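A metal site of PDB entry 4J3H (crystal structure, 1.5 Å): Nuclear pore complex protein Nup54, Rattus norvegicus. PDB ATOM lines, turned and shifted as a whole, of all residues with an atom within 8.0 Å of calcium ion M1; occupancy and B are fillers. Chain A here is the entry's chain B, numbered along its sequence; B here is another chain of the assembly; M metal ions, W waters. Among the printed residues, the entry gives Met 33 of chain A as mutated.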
ATOM      1  N   LEU A  32     -24.090 -22.705   7.435  1.00  0.00           N
ATOM      2  CA  LEU A  32     -24.283 -21.272   7.193  1.00  0.00           C
ATOM      3  C   LEU A  32     -23.883 -20.861   5.780  1.00  0.00           C
ATOM      4  O   LEU A  32     -24.544 -20.040   5.162  1.00  0.00           O
ATOM      5  CB  LEU A  32     -23.552 -20.407   8.239  1.00  0.00           C
ATOM      6  CG  LEU A  32     -24.071 -20.522   9.681  1.00  0.00           C
ATOM      7  CD1 LEU A  32     -23.201 -19.688  10.634  1.00  0.00           C
ATOM      8  CD2 LEU A  32     -25.530 -20.128   9.761  1.00  0.00           C
ATOM      9  N   MET A  33     -22.791 -21.440   5.272  1.00  0.00           N
ATOM     10  CA  MET A  33     -22.388 -21.148   3.901  1.00  0.00           C
ATOM     11  C   MET A  33     -23.474 -21.485   2.902  1.00  0.00           C
ATOM     12  O   MET A  33     -23.590 -20.828   1.860  1.00  0.00           O
ATOM     13  CB  MET A  33     -21.114 -21.901   3.561  1.00  0.00           C
ATOM     14  CG  MET A  33     -19.904 -21.411   4.331  1.00  0.00           C
ATOM     15  SD  MET A  33     -19.585 -19.520   4.004  1.00  0.00           S
ATOM     16  CE  MET A  33     -19.906 -19.589   2.098  1.00  0.00           C
ATOM     17  N   SER A  34     -24.256 -22.522   3.188  1.00  0.00           N
ATOM     18  CA  SER A  34     -25.316 -22.921   2.265  1.00  0.00           C
ATOM     19  C   SER A  34     -26.429 -21.885   2.220  1.00  0.00           C
ATOM     20  O   SER A  34     -27.315 -21.971   1.341  1.00  0.00           O
ATOM     21  CB  SER A  34     -25.903 -24.273   2.657  1.00  0.00           C
ATOM     22  OG  SER A  34     -26.821 -24.167   3.724  1.00  0.00           O
ATOM     23  N   ILE A  35     -26.393 -20.907   3.117  1.00  0.00           N
ATOM     24  CA  ILE A  35     -27.377 -19.829   3.143  1.00  0.00           C
ATOM     25  C   ILE A  35     -26.768 -18.517   2.635  1.00  0.00           C
ATOM     26  O   ILE A  35     -27.373 -17.804   1.822  1.00  0.00           O
ATOM     27  CB  ILE A  35     -27.927 -19.600   4.587  1.00  0.00           C
ATOM     28  CG1 ILE A  35     -28.283 -20.944   5.218  1.00  0.00           C
ATOM     29  CG2 ILE A  35     -29.079 -18.604   4.589  1.00  0.00           C
ATOM     30  CD1 ILE A  35     -28.732 -20.865   6.665  1.00  0.00           C
ATOM     31  N   ILE A  36     -25.542 -18.228   3.095  1.00  0.00           N
ATOM     32  CA  ILE A  36     -24.953 -16.911   2.914  1.00  0.00           C
ATOM     33  C   ILE A  36     -23.979 -16.808   1.760  1.00  0.00           C
ATOM     34  O   ILE A  36     -23.652 -15.705   1.350  1.00  0.00           O
ATOM     35  CB  ILE A  36     -24.282 -16.409   4.237  1.00  0.00           C
ATOM     36  CG1 ILE A  36     -24.212 -14.881   4.276  1.00  0.00           C
ATOM     37  CG2 ILE A  36     -22.927 -17.089   4.451  1.00  0.00           C
ATOM     38  CD1 ILE A  36     -23.657 -14.335   5.617  1.00  0.00           C
ATOM     39  N   LYS A  37     -23.511 -17.930   1.219  1.00  0.00           N
ATOM     40  CA  LYS A  37     -22.492 -17.881   0.156  1.00  0.00           C
ATOM     41  C   LYS A  37     -22.896 -17.017  -1.037  1.00  0.00           C
ATOM     42  O   LYS A  37     -22.125 -16.177  -1.483  1.00  0.00           O
ATOM     43  CB  LYS A  37     -22.078 -19.281  -0.309  1.00  0.00           C
ATOM     44  CG  LYS A  37     -21.093 -19.290  -1.460  1.00  0.00           C
ATOM     45  CD  LYS A  37     -20.826 -20.720  -1.957  1.00  0.00           C
ATOM     46  CE  LYS A  37     -20.054 -20.728  -3.281  1.00  0.00           C
ATOM     47  NZ  LYS A  37     -18.685 -20.195  -3.103  1.00  0.00           N
ATOM     48  N   ASP A  38     -24.125 -17.187  -1.539  1.00  0.00           N
ATOM     49  CA  ASP A  38     -24.542 -16.418  -2.710  1.00  0.00           C
ATOM     50  C   ASP A  38     -24.773 -14.933  -2.414  1.00  0.00           C
ATOM     51  O   ASP A  38     -24.861 -14.114  -3.331  1.00  0.00           O
ATOM     52  CB  ASP A  38     -25.750 -17.048  -3.432  1.00  0.00           C
ATOM     53  CG  ASP A  38     -26.951 -17.207  -2.535  1.00  0.00           C
ATOM     54  OD1 ASP A  38     -26.901 -16.659  -1.431  1.00  0.00           O
ATOM     55  OD2 ASP A  38     -27.944 -17.873  -2.934  1.00  0.00           O
ATOM     56  N   ASP A  39     -24.877 -14.581  -1.135  1.00  0.00           N
ATOM     57  CA  ASP A  39     -24.981 -13.177  -0.757  1.00  0.00           C
ATOM     58  C   ASP A  39     -23.603 -12.525  -0.681  1.00  0.00           C
ATOM     59  O   ASP A  39     -23.447 -11.363  -1.051  1.00  0.00           O
ATOM     60  CB  ASP A  39     -25.751 -13.036   0.559  1.00  0.00           C
ATOM     61  CG  ASP A  39     -27.161 -13.560   0.438  1.00  0.00           C
ATOM     62  OD1 ASP A  39     -28.008 -12.869  -0.165  1.00  0.00           O
ATOM     63  OD2 ASP A  39     -27.390 -14.673   0.926  1.00  0.00           O
ATOM     64  N   LEU A  40     -22.607 -13.288  -0.228  1.00  0.00           N
ATOM     65  CA  LEU A  40     -21.230 -12.800  -0.201  1.00  0.00           C
ATOM     66  C   LEU A  40     -20.738 -12.498  -1.616  1.00  0.00           C
ATOM     67  O   LEU A  40     -19.872 -11.626  -1.802  1.00  0.00           O
ATOM     68  CB  LEU A  40     -20.300 -13.821   0.453  1.00  0.00           C
ATOM     69  CG  LEU A  40     -20.680 -14.281   1.861  1.00  0.00           C
ATOM     70  CD1 LEU A  40     -19.660 -15.272   2.413  1.00  0.00           C
ATOM     71  CD2 LEU A  40     -20.834 -13.082   2.792  1.00  0.00           C
ATOM     72  N   ASP A  42     -22.900 -11.850  -4.355  1.00  0.00           N
ATOM     73  CA  ASP A  42     -23.807 -10.969  -5.080  1.00  0.00           C
ATOM     74  C   ASP A  42     -25.012 -10.583  -4.224  1.00  0.00           C
ATOM     75  O   ASP A  42     -26.086 -11.157  -4.344  1.00  0.00           O
ATOM     76  N   ASP B  11     -32.438 -11.425   5.944  1.00  0.00           N
ATOM     77  CA  ASP B  11     -33.642 -12.251   6.035  1.00  0.00           C
ATOM     78  C   ASP B  11     -33.712 -12.983   7.370  1.00  0.00           C
ATOM     79  O   ASP B  11     -32.679 -13.400   7.951  1.00  0.00           O
ATOM     80  CB  ASP B  11     -33.725 -13.303   4.900  1.00  0.00           C
ATOM     81  CG  ASP B  11     -34.250 -12.759   3.598  1.00  0.00           C
ATOM     82  OD1 ASP B  11     -34.074 -11.595   3.284  1.00  0.00           O
ATOM     83  OD2 ASP B  11     -34.814 -13.578   2.859  1.00  0.00           O
ATOM     84  N   ASP B  13     -34.594 -16.047   8.176  1.00  0.00           N
ATOM     85  CA  ASP B  13     -34.035 -17.400   8.251  1.00  0.00           C
ATOM     86  C   ASP B  13     -32.528 -17.375   8.459  1.00  0.00           C
ATOM     87  O   ASP B  13     -31.990 -18.097   9.309  1.00  0.00           O
ATOM     88  CB  ASP B  13     -34.505 -18.333   7.117  1.00  0.00           C
ATOM     89  CG  ASP B  13     -34.311 -17.790   5.720  1.00  0.00           C
ATOM     90  OD1 ASP B  13     -33.670 -16.745   5.482  1.00  0.00           O
ATOM     91  OD2 ASP B  13     -34.819 -18.483   4.786  1.00  0.00           O
ATOM     92  N   LEU B  14     -31.819 -16.544   7.691  1.00  0.00           N
ATOM     93  CA  LEU B  14     -30.378 -16.434   7.870  1.00  0.00           C
ATOM     94  C   LEU B  14     -30.036 -15.945   9.265  1.00  0.00           C
ATOM     95  O   LEU B  14     -29.138 -16.501   9.921  1.00  0.00           O
ATOM     96  CB  LEU B  14     -29.777 -15.526   6.796  1.00  0.00           C
ATOM     97  CG  LEU B  14     -28.264 -15.250   6.966  1.00  0.00           C
ATOM     98  CD1 LEU B  14     -27.473 -16.527   7.056  1.00  0.00           C
ATOM     99  CD2 LEU B  14     -27.730 -14.393   5.820  1.00  0.00           C
HETATM  100 CA    CA M   1     -28.575 -16.640   0.318  1.00  0.00          CA
HETATM  101 CA    CA M   2     -34.884 -11.903   0.887  1.00  0.00          CA
HETATM  102  O   HOH W   1     -29.180 -18.726  -0.616  1.00  0.00           O
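Of the 13 residues printed, 3 come within 4 Å of calcium ion M1.
The nearest printed residue that does not touch calcium ion M1 is Ile 36 (4.4 Å).
The backbone carbonyl oxygen (O) of Ile 35 binds calcium ion M1, at 2.2 Å.
Water W1 binds calcium ion M1, at 2.4 Å.
OD2 of Asp 39 is bound to calcium ion M1.
OD1 of Asp 38 binds calcium ion M1 (2.4 Å).
Calcium ion M1 has four donor atoms within binding distance.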
